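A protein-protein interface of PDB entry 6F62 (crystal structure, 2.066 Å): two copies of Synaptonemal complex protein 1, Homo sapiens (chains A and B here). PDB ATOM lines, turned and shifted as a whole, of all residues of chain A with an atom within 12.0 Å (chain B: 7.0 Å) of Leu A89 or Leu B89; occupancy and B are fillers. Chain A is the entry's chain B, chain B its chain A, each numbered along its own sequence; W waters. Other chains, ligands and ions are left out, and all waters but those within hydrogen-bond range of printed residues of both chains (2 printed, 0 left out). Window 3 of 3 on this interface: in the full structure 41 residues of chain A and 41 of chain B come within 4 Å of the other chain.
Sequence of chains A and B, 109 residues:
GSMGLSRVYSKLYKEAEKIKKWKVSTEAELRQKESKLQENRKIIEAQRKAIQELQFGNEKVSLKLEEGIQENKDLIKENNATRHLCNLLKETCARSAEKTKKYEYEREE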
ATOM      1  N   ASN A  79     -13.339  35.033 -17.235  1.00  0.00           N
ATOM      2  CA  ASN A  79     -13.482  33.812 -16.447  1.00  0.00           C
ATOM      3  C   ASN A  79     -14.344  34.049 -15.212  1.00  0.00           C
ATOM      4  O   ASN A  79     -15.135  33.182 -14.823  1.00  0.00           O
ATOM      5  CB  ASN A  79     -12.107  33.274 -16.048  1.00  0.00           C
ATOM      6  CG  ASN A  79     -11.615  32.183 -16.980  1.00  0.00           C
ATOM      7  OD1 ASN A  79     -12.093  31.049 -16.933  1.00  0.00           O
ATOM      8  ND2 ASN A  79     -10.651  32.518 -17.833  1.00  0.00           N
ATOM      9  N   ASN A  80     -14.207  35.219 -14.584  1.00  0.00           N
ATOM     10  CA  ASN A  80     -15.023  35.529 -13.414  1.00  0.00           C
ATOM     11  C   ASN A  80     -16.505  35.522 -13.762  1.00  0.00           C
ATOM     12  O   ASN A  80     -17.326  34.960 -13.030  1.00  0.00           O
ATOM     13  CB  ASN A  80     -14.619  36.884 -12.834  1.00  0.00           C
ATOM     14  CG  ASN A  80     -13.318  36.826 -12.061  1.00  0.00           C
ATOM     15  OD1 ASN A  80     -12.821  35.747 -11.736  1.00  0.00           O
ATOM     16  ND2 ASN A  80     -12.763  37.992 -11.750  1.00  0.00           N
ATOM     17  N   ALA A  81     -16.867  36.150 -14.882  1.00  0.00           N
ATOM     18  CA  ALA A  81     -18.272  36.213 -15.270  1.00  0.00           C
ATOM     19  C   ALA A  81     -18.815  34.830 -15.605  1.00  0.00           C
ATOM     20  O   ALA A  81     -19.965  34.512 -15.278  1.00  0.00           O
ATOM     21  CB  ALA A  81     -18.444  37.161 -16.457  1.00  0.00           C
ATOM     22  N   THR A  82     -18.005  33.992 -16.257  1.00  0.00           N
ATOM     23  CA  THR A  82     -18.460  32.651 -16.611  1.00  0.00           C
ATOM     24  C   THR A  82     -18.621  31.779 -15.371  1.00  0.00           C
ATOM     25  O   THR A  82     -19.527  30.940 -15.310  1.00  0.00           O
ATOM     26  CB  THR A  82     -17.486  32.009 -17.600  1.00  0.00           C
ATOM     27  OG1 THR A  82     -17.297  32.883 -18.719  1.00  0.00           O
ATOM     28  CG2 THR A  82     -18.021  30.676 -18.100  1.00  0.00           C
ATOM     29  N   ARG A  83     -17.750  31.958 -14.375  1.00  0.00           N
ATOM     30  CA  ARG A  83     -17.895  31.224 -13.121  1.00  0.00           C
ATOM     31  C   ARG A  83     -19.198  31.594 -12.422  1.00  0.00           C
ATOM     32  O   ARG A  83     -19.934  30.720 -11.951  1.00  0.00           O
ATOM     33  CB  ARG A  83     -16.702  31.507 -12.207  1.00  0.00           C
ATOM     34  CG  ARG A  83     -15.445  30.717 -12.533  1.00  0.00           C
ATOM     35  CD  ARG A  83     -14.293  31.159 -11.643  1.00  0.00           C
ATOM     36  NE  ARG A  83     -13.095  30.340 -11.818  1.00  0.00           N
ATOM     37  CZ  ARG A  83     -12.828  29.230 -11.131  1.00  0.00           C
ATOM     38  NH1 ARG A  83     -13.673  28.782 -10.211  1.00  0.00           N
ATOM     39  NH2 ARG A  83     -11.707  28.564 -11.368  1.00  0.00           N
ATOM     40  N   HIS A  84     -19.496  32.892 -12.342  1.00  0.00           N
ATOM     41  CA  HIS A  84     -20.715  33.336 -11.672  1.00  0.00           C
ATOM     42  C   HIS A  84     -21.949  32.725 -12.325  1.00  0.00           C
ATOM     43  O   HIS A  84     -22.844  32.221 -11.637  1.00  0.00           O
ATOM     44  CB  HIS A  84     -20.790  34.864 -11.691  1.00  0.00           C
ATOM     45  CG  HIS A  84     -22.009  35.417 -11.020  1.00  0.00           C
ATOM     46  ND1 HIS A  84     -22.378  35.066  -9.740  1.00  0.00           N
ATOM     47  CD2 HIS A  84     -22.942  36.299 -11.452  1.00  0.00           C
ATOM     48  CE1 HIS A  84     -23.487  35.705  -9.412  1.00  0.00           C
ATOM     49  NE2 HIS A  84     -23.850  36.460 -10.433  1.00  0.00           N
ATOM     50  N   LEU A  85     -22.014  32.759 -13.658  1.00  0.00           N
ATOM     51  CA  LEU A  85     -23.136  32.139 -14.356  1.00  0.00           C
ATOM     52  C   LEU A  85     -23.192  30.643 -14.075  1.00  0.00           C
ATOM     53  O   LEU A  85     -24.274  30.079 -13.876  1.00  0.00           O
ATOM     54  CB  LEU A  85     -23.027  32.399 -15.859  1.00  0.00           C
ATOM     55  CG  LEU A  85     -24.042  31.675 -16.747  1.00  0.00           C
ATOM     56  CD1 LEU A  85     -25.468  32.003 -16.329  1.00  0.00           C
ATOM     57  CD2 LEU A  85     -23.817  32.032 -18.209  1.00  0.00           C
ATOM     58  N   CYS A  86     -22.032  29.984 -14.057  1.00  0.00           N
ATOM     59  CA  CYS A  86     -21.994  28.553 -13.779  1.00  0.00           C
ATOM     60  C   CYS A  86     -22.566  28.243 -12.401  1.00  0.00           C
ATOM     61  O   CYS A  86     -23.338  27.291 -12.239  1.00  0.00           O
ATOM     62  CB  CYS A  86     -20.557  28.044 -13.894  1.00  0.00           C
ATOM     63  SG  CYS A  86     -20.400  26.253 -13.950  1.00  0.00           S
ATOM     64  N   ASN A  87     -22.199  29.041 -11.393  1.00  0.00           N
ATOM     65  CA  ASN A  87     -22.700  28.805 -10.042  1.00  0.00           C
ATOM     66  C   ASN A  87     -24.211  28.985  -9.969  1.00  0.00           C
ATOM     67  O   ASN A  87     -24.906  28.198  -9.314  1.00  0.00           O
ATOM     68  CB  ASN A  87     -21.999  29.738  -9.054  1.00  0.00           C
ATOM     69  CG  ASN A  87     -20.567  29.324  -8.778  1.00  0.00           C
ATOM     70  OD1 ASN A  87     -20.217  28.148  -8.889  1.00  0.00           O
ATOM     71  ND2 ASN A  87     -19.730  30.289  -8.417  1.00  0.00           N
ATOM     72  N   LEU A  88     -24.742  30.018 -10.629  1.00  0.00           N
ATOM     73  CA  LEU A  88     -26.189  30.201 -10.674  1.00  0.00           C
ATOM     74  C   LEU A  88     -26.875  28.967 -11.247  1.00  0.00           C
ATOM     75  O   LEU A  88     -27.877  28.487 -10.702  1.00  0.00           O
ATOM     76  CB  LEU A  88     -26.541  31.439 -11.502  1.00  0.00           C
ATOM     77  CG  LEU A  88     -26.049  32.798 -10.997  1.00  0.00           C
ATOM     78  CD1 LEU A  88     -26.588  33.908 -11.888  1.00  0.00           C
ATOM     79  CD2 LEU A  88     -26.445  33.036  -9.546  1.00  0.00           C
ATOM     80  N   LEU A  89     -26.347  28.438 -12.353  1.00  0.00           N
ATOM     81  CA  LEU A  89     -26.949  27.261 -12.969  1.00  0.00           C
ATOM     82  C   LEU A  89     -26.870  26.054 -12.042  1.00  0.00           C
ATOM     83  O   LEU A  89     -27.801  25.242 -11.990  1.00  0.00           O
ATOM     84  CB  LEU A  89     -26.264  26.962 -14.302  1.00  0.00           C
ATOM     85  CG  LEU A  89     -26.582  27.936 -15.437  1.00  0.00           C
ATOM     86  CD1 LEU A  89     -25.585  27.774 -16.577  1.00  0.00           C
ATOM     87  CD2 LEU A  89     -28.006  27.732 -15.938  1.00  0.00           C
ATOM     88  N   LYS A  90     -25.767  25.917 -11.302  1.00  0.00           N
ATOM     89  CA  LYS A  90     -25.648  24.810 -10.359  1.00  0.00           C
ATOM     90  C   LYS A  90     -26.732  24.879  -9.290  1.00  0.00           C
ATOM     91  O   LYS A  90     -27.325  23.856  -8.931  1.00  0.00           O
ATOM     92  CB  LYS A  90     -24.261  24.813  -9.714  1.00  0.00           C
ATOM     93  CG  LYS A  90     -23.153  24.289 -10.614  1.00  0.00           C
ATOM     94  CD  LYS A  90     -21.813  24.279  -9.896  1.00  0.00           C
ATOM     95  CE  LYS A  90     -20.725  23.643 -10.750  1.00  0.00           C
ATOM     96  NZ  LYS A  90     -19.371  23.788 -10.144  1.00  0.00           N
ATOM     97  N   GLU A  91     -27.003  26.077  -8.767  1.00  0.00           N
ATOM     98  CA  GLU A  91     -28.040  26.223  -7.749  1.00  0.00           C
ATOM     99  C   GLU A  91     -29.407  25.842  -8.304  1.00  0.00           C
ATOM    100  O   GLU A  91     -30.176  25.122  -7.656  1.00  0.00           O
ATOM    101  CB  GLU A  91     -28.059  27.655  -7.216  1.00  0.00           C
ATOM    102  CG  GLU A  91     -26.980  27.954  -6.192  1.00  0.00           C
ATOM    103  CD  GLU A  91     -27.220  29.263  -5.465  1.00  0.00           C
ATOM    104  OE1 GLU A  91     -28.152  29.998  -5.854  1.00  0.00           O
ATOM    105  OE2 GLU A  91     -26.480  29.556  -4.504  1.00  0.00           O
ATOM    106  N   THR A  92     -29.729  26.324  -9.505  1.00  0.00           N
ATOM    107  CA  THR A  92     -31.007  25.981 -10.120  1.00  0.00           C
ATOM    108  C   THR A  92     -31.142  24.475 -10.302  1.00  0.00           C
ATOM    109  O   THR A  92     -32.219  23.908 -10.078  1.00  0.00           O
ATOM    110  CB  THR A  92     -31.149  26.700 -11.464  1.00  0.00           C
ATOM    111  OG1 THR A  92     -31.016  28.113 -11.267  1.00  0.00           O
ATOM    112  CG2 THR A  92     -32.504  26.412 -12.100  1.00  0.00           C
ATOM    113  N   CYS A  93     -30.059  23.806 -10.703  1.00  0.00           N
ATOM    114  CA  CYS A  93     -30.114  22.361 -10.905  1.00  0.00           C
ATOM    115  C   CYS A  93     -30.384  21.633  -9.596  1.00  0.00           C
ATOM    116  O   CYS A  93     -31.292  20.799  -9.511  1.00  0.00           O
ATOM    117  CB  CYS A  93     -28.810  21.868 -11.535  1.00  0.00           C
ATOM    118  SG  CYS A  93     -28.788  21.978 -13.335  1.00  0.00           S
ATOM    119  N   ALA A  94     -29.598  21.933  -8.560  1.00  0.00           N
ATOM    120  CA  ALA A  94     -29.769  21.258  -7.278  1.00  0.00           C
ATOM    121  C   ALA A  94     -31.175  21.469  -6.730  1.00  0.00           C
ATOM    122  O   ALA A  94     -31.847  20.515  -6.322  1.00  0.00           O
ATOM    123  CB  ALA A  94     -28.722  21.758  -6.283  1.00  0.00           C
ATOM    124  N   ARG A  95     -31.639  22.721  -6.713  1.00  0.00           N
ATOM    125  CA  ARG A  95     -32.974  23.011  -6.202  1.00  0.00           C
ATOM    126  C   ARG A  95     -34.041  22.285  -7.012  1.00  0.00           C
ATOM    127  O   ARG A  95     -35.007  21.759  -6.450  1.00  0.00           O
ATOM    128  CB  ARG A  95     -33.216  24.522  -6.215  1.00  0.00           C
ATOM    129  CG  ARG A  95     -34.591  24.959  -5.709  1.00  0.00           C
ATOM    130  CD  ARG A  95     -35.643  25.001  -6.813  1.00  0.00           C
ATOM    131  NE  ARG A  95     -35.234  25.839  -7.936  1.00  0.00           N
ATOM    132  CZ  ARG A  95     -35.798  25.811  -9.139  1.00  0.00           C
ATOM    133  NH1 ARG A  95     -36.797  24.976  -9.392  1.00  0.00           N
ATOM    134  NH2 ARG A  95     -35.357  26.615 -10.095  1.00  0.00           N
ATOM    135  N   SER A  96     -33.890  22.256  -8.338  1.00  0.00           N
ATOM    136  CA  SER A  96     -34.881  21.592  -9.175  1.00  0.00           C
ATOM    137  C   SER A  96     -34.844  20.081  -8.995  1.00  0.00           C
ATOM    138  O   SER A  96     -35.883  19.420  -9.103  1.00  0.00           O
ATOM    139  CB  SER A  96     -34.654  21.962 -10.641  1.00  0.00           C
ATOM    140  OG  SER A  96     -35.623  21.355 -11.478  1.00  0.00           O
ATOM    141  N   ALA A  97     -33.666  19.518  -8.717  1.00  0.00           N
ATOM    142  CA  ALA A  97     -33.560  18.071  -8.556  1.00  0.00           C
ATOM    143  C   ALA A  97     -34.201  17.609  -7.252  1.00  0.00           C
ATOM    144  O   ALA A  97     -34.841  16.552  -7.211  1.00  0.00           O
ATOM    145  CB  ALA A  97     -32.096  17.643  -8.615  1.00  0.00           C
ATOM    146  N   GLU A  98     -34.041  18.382  -6.175  1.00  0.00           N
ATOM    147  CA  GLU A  98     -34.663  18.003  -4.909  1.00  0.00           C
ATOM    148  C   GLU A  98     -36.178  18.142  -4.985  1.00  0.00           C
ATOM    149  O   GLU A  98     -36.911  17.341  -4.392  1.00  0.00           O
ATOM    150  CB  GLU A  98     -34.091  18.845  -3.763  1.00  0.00           C
ATOM    151  CG  GLU A  98     -34.769  20.192  -3.543  1.00  0.00           C
ATOM    152  CD  GLU A  98     -34.098  21.011  -2.454  1.00  0.00           C
ATOM    153  OE1 GLU A  98     -33.008  20.610  -1.990  1.00  0.00           O
ATOM    154  OE2 GLU A  98     -34.660  22.054  -2.059  1.00  0.00           O
ATOM    155  N   THR B  82     -15.450  25.983 -18.774  1.00  0.00           N
ATOM    156  CA  THR B  82     -16.566  26.412 -17.940  1.00  0.00           C
ATOM    157  C   THR B  82     -17.795  26.721 -18.789  1.00  0.00           C
ATOM    158  O   THR B  82     -18.928  26.449 -18.373  1.00  0.00           O
ATOM    159  CB  THR B  82     -16.164  27.629 -17.105  1.00  0.00           C
ATOM    160  OG1 THR B  82     -14.901  27.382 -16.476  1.00  0.00           O
ATOM    161  CG2 THR B  82     -17.203  27.902 -16.024  1.00  0.00           C
ATOM    162  N   HIS B  84     -18.560  25.128 -21.524  1.00  0.00           N
ATOM    163  CA  HIS B  84     -19.115  23.813 -21.823  1.00  0.00           C
ATOM    164  C   HIS B  84     -19.927  23.284 -20.648  1.00  0.00           C
ATOM    165  O   HIS B  84     -21.032  22.758 -20.832  1.00  0.00           O
ATOM    166  CB  HIS B  84     -17.992  22.840 -22.183  1.00  0.00           C
ATOM    167  CG  HIS B  84     -18.474  21.464 -22.512  1.00  0.00           C
ATOM    168  ND1 HIS B  84     -19.419  21.220 -23.486  1.00  0.00           N
ATOM    169  CD2 HIS B  84     -18.147  20.256 -21.995  1.00  0.00           C
ATOM    170  CE1 HIS B  84     -19.652  19.921 -23.555  1.00  0.00           C
ATOM    171  NE2 HIS B  84     -18.893  19.314 -22.661  1.00  0.00           N
ATOM    172  N   LEU B  85     -19.401  23.422 -19.430  1.00  0.00           N
ATOM    173  CA  LEU B  85     -20.139  22.980 -18.252  1.00  0.00           C
ATOM    174  C   LEU B  85     -21.453  23.738 -18.113  1.00  0.00           C
ATOM    175  O   LEU B  85     -22.477  23.155 -17.740  1.00  0.00           O
ATOM    176  CB  LEU B  85     -19.278  23.153 -17.002  1.00  0.00           C
ATOM    177  CG  LEU B  85     -19.899  22.711 -15.676  1.00  0.00           C
ATOM    178  CD1 LEU B  85     -20.309  21.244 -15.726  1.00  0.00           C
ATOM    179  CD2 LEU B  85     -18.922  22.955 -14.535  1.00  0.00           C
ATOM    180  N   CYS B  86     -21.447  25.041 -18.408  1.00  0.00           N
ATOM    181  CA  CYS B  86     -22.688  25.808 -18.372  1.00  0.00           C
ATOM    182  C   CYS B  86     -23.734  25.206 -19.302  1.00  0.00           C
ATOM    183  O   CYS B  86     -24.908  25.082 -18.931  1.00  0.00           O
ATOM    184  CB  CYS B  86     -22.420  27.268 -18.746  1.00  0.00           C
ATOM    185  SG  CYS B  86     -21.631  28.248 -17.445  1.00  0.00           S
ATOM    186  N   ASN B  87     -23.330  24.819 -20.513  1.00  0.00           N
ATOM    187  CA  ASN B  87     -24.289  24.262 -21.461  1.00  0.00           C
ATOM    188  C   ASN B  87     -24.842  22.930 -20.969  1.00  0.00           C
ATOM    189  O   ASN B  87     -26.026  22.634 -21.168  1.00  0.00           O
ATOM    190  CB  ASN B  87     -23.637  24.107 -22.833  1.00  0.00           C
ATOM    191  CG  ASN B  87     -23.463  25.437 -23.544  1.00  0.00           C
ATOM    192  OD1 ASN B  87     -24.171  26.401 -23.256  1.00  0.00           O
ATOM    193  ND2 ASN B  87     -22.519  25.495 -24.474  1.00  0.00           N
ATOM    194  N   LEU B  88     -24.008  22.113 -20.323  1.00  0.00           N
ATOM    195  CA  LEU B  88     -24.500  20.857 -19.765  1.00  0.00           C
ATOM    196  C   LEU B  88     -25.527  21.112 -18.667  1.00  0.00           C
ATOM    197  O   LEU B  88     -26.585  20.471 -18.633  1.00  0.00           O
ATOM    198  CB  LEU B  88     -23.332  20.026 -19.229  1.00  0.00           C
ATOM    199  CG  LEU B  88     -22.286  19.584 -20.256  1.00  0.00           C
ATOM    200  CD1 LEU B  88     -21.143  18.855 -19.570  1.00  0.00           C
ATOM    201  CD2 LEU B  88     -22.902  18.706 -21.336  1.00  0.00           C
ATOM    202  N   LEU B  89     -25.237  22.050 -17.762  1.00  0.00           N
ATOM    203  CA  LEU B  89     -26.181  22.361 -16.695  1.00  0.00           C
ATOM    204  C   LEU B  89     -27.510  22.856 -17.251  1.00  0.00           C
ATOM    205  O   LEU B  89     -28.567  22.574 -16.675  1.00  0.00           O
ATOM    206  CB  LEU B  89     -25.576  23.396 -15.747  1.00  0.00           C
ATOM    207  CG  LEU B  89     -24.346  22.937 -14.958  1.00  0.00           C
ATOM    208  CD1 LEU B  89     -23.692  24.114 -14.248  1.00  0.00           C
ATOM    209  CD2 LEU B  89     -24.723  21.856 -13.956  1.00  0.00           C
ATOM    210  N   LYS B  90     -27.486  23.588 -18.367  1.00  0.00           N
ATOM    211  CA  LYS B  90     -28.735  24.028 -18.980  1.00  0.00           C
ATOM    212  C   LYS B  90     -29.553  22.840 -19.470  1.00  0.00           C
ATOM    213  O   LYS B  90     -30.783  22.829 -19.340  1.00  0.00           O
ATOM    214  CB  LYS B  90     -28.447  24.990 -20.132  1.00  0.00           C
ATOM    215  CG  LYS B  90     -27.937  26.356 -19.694  1.00  0.00           C
ATOM    216  CD  LYS B  90     -27.681  27.253 -20.896  1.00  0.00           C
ATOM    217  CE  LYS B  90     -27.163  28.622 -20.486  1.00  0.00           C
ATOM    218  NZ  LYS B  90     -27.049  29.541 -21.654  1.00  0.00           N
ATOM    219  N   GLU B  91     -28.891  21.832 -20.044  1.00  0.00           N
ATOM    220  CA  GLU B  91     -29.598  20.625 -20.460  1.00  0.00           C
ATOM    221  C   GLU B  91     -30.270  19.952 -19.271  1.00  0.00           C
ATOM    222  O   GLU B  91     -31.430  19.533 -19.350  1.00  0.00           O
ATOM    223  CB  GLU B  91     -28.632  19.654 -21.141  1.00  0.00           C
ATOM    224  CG  GLU B  91     -27.995  20.183 -22.413  1.00  0.00           C
ATOM    225  CD  GLU B  91     -27.138  19.140 -23.107  1.00  0.00           C
ATOM    226  OE1 GLU B  91     -27.334  17.934 -22.839  1.00  0.00           O
ATOM    227  OE2 GLU B  91     -26.266  19.522 -23.916  1.00  0.00           O
ATOM    228  N   THR B  92     -29.546  19.834 -18.154  1.00  0.00           N
ATOM    229  CA  THR B  92     -30.117  19.225 -16.957  1.00  0.00           C
ATOM    230  C   THR B  92     -31.329  20.007 -16.468  1.00  0.00           C
ATOM    231  O   THR B  92     -32.352  19.417 -16.105  1.00  0.00           O
ATOM    232  CB  THR B  92     -29.055  19.138 -15.860  1.00  0.00           C
ATOM    233  OG1 THR B  92     -27.892  18.473 -16.372  1.00  0.00           O
ATOM    234  CG2 THR B  92     -29.583  18.372 -14.652  1.00  0.00           C
ATOM    235  N   CYS B  93     -31.231  21.341 -16.447  1.00  0.00           N
ATOM    236  CA  CYS B  93     -32.374  22.161 -16.060  1.00  0.00           C
ATOM    237  C   CYS B  93     -33.579  21.881 -16.945  1.00  0.00           C
ATOM    238  O   CYS B  93     -34.710  21.781 -16.456  1.00  0.00           O
ATOM    239  CB  CYS B  93     -32.009  23.644 -16.133  1.00  0.00           C
ATOM    240  SG  CYS B  93     -30.997  24.237 -14.764  1.00  0.00           S
ATOM    241  N   ALA B  94     -33.357  21.757 -18.255  1.00  0.00           N
ATOM    242  CA  ALA B  94     -34.465  21.577 -19.186  1.00  0.00           C
ATOM    243  C   ALA B  94     -35.247  20.308 -18.872  1.00  0.00           C
ATOM    244  O   ALA B  94     -36.480  20.333 -18.781  1.00  0.00           O
ATOM    245  CB  ALA B  94     -33.937  21.546 -20.620  1.00  0.00           C
HETATM  246  O   HOH W   1     -14.480  30.777 -15.859  1.00  0.00           O
HETATM  247  O   HOH W   2     -13.324  28.774 -14.592  1.00  0.00           O
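Cys A86 touches Leu B85, but with the chains exchanged Leu A85 does not touch Cys B86 (4.2 Å). Cys A86 touches its own counterpart, Cys B86. Cys A86 touches Leu B89, and with the chains exchanged Leu A89 touches Cys B86. Cys A93 touches Leu B89, but with the chains exchanged Leu A89 does not touch Cys B93 (4.3 Å). Positions printed for both chains: 82, 84, 85, 86, 87, 88, 89, 90, 91, 92, 93 and 94.
SG of Cys B93 is in hydrogen-bond range of O of Leu B89 (3.5 Å). The side-chain sulfur (SG) of Cys A93 sits close to the backbone carbonyl oxygen (O) of Leu A89 (3.7 Å). The backbone carbonyl oxygen (O) of Thr B82 is in hydrogen-bond range of the side-chain sulfur (SG) of Cys B86 (3.4 Å). O of Leu B88 sits at hydrogen-bond distance from OG1 of Thr B92, 3.3 Å away. The backbone carbonyl oxygen (O) of Leu A88 sits at hydrogen-bond distance from the side-chain hydroxyl (OG1) of Thr A92, at 3.2 Å.
The side-chain sulfur of Cys B93 lies within hydrogen-bond range of the side-chain sulfur of Cys A93 (3.5 Å). SG of Cys A93 is in hydrogen-bond range of O of Leu B89, 3.4 Å away.
Among the printed residues, pairs that only touch across the chains: Thr A82 with Thr B82, Leu A89 with Cys B86, Cys A86 with Leu B85, Lys A90 with Leu B89, Cys A86 with Cys B86, Thr A92 with Cys B93, Cys A86 with Leu B89, Cys A93 with Thr B92, Leu A89 with Leu B89 and Cys A86 with Thr B82.
Hydrophobic or aromatic side chains of chain A that line the printed part of chain B: Leu A89. Among the printed residues, 12 pairs touch across the chains. Among the printed residues, no Asp or Glu carboxylate lies within 4 Å of a Lys or Arg side-chain nitrogen of the other chain.
Water W1 lies within hydrogen-bond range of the side-chain amide oxygen (OD1) of Asn A79 (2.6 Å) and the side-chain hydroxyl (OG1) of Thr B82 (3.5 Å). Water W2 lies within hydrogen-bond range of the side-chain hydroxyl of Thr B82 (2.8 Å), the guanidinium group of Arg A83 (3.2 Å) and the side-chain amide oxygen of Asn A79 (3.5 Å).
Leu B89 touches just these residues of chain A: Cys A86, Leu A89, Lys A90 and Cys A93. Of the printed residues of chain A, Leu B85 touches Cys A86. No residue of chain A comes within 4 Å of Glu B91. Of chain A, only Thr A92 (3.8 Å) and Cys A93 (3.5 Å) come within 4 Å of Cys B93. Printed residues of chain B within 4 Å of Thr A82: Thr B82 (3.6 Å). Of the printed residues of chain B, Cys A93 touches Leu B89 (3.4 Å), Thr B92 (3.8 Å) and Cys B93 (3.5 Å). Of the printed residues of chain B, Thr A92 touches Cys B93. Glu A98 touches none of the printed residues of chain B.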
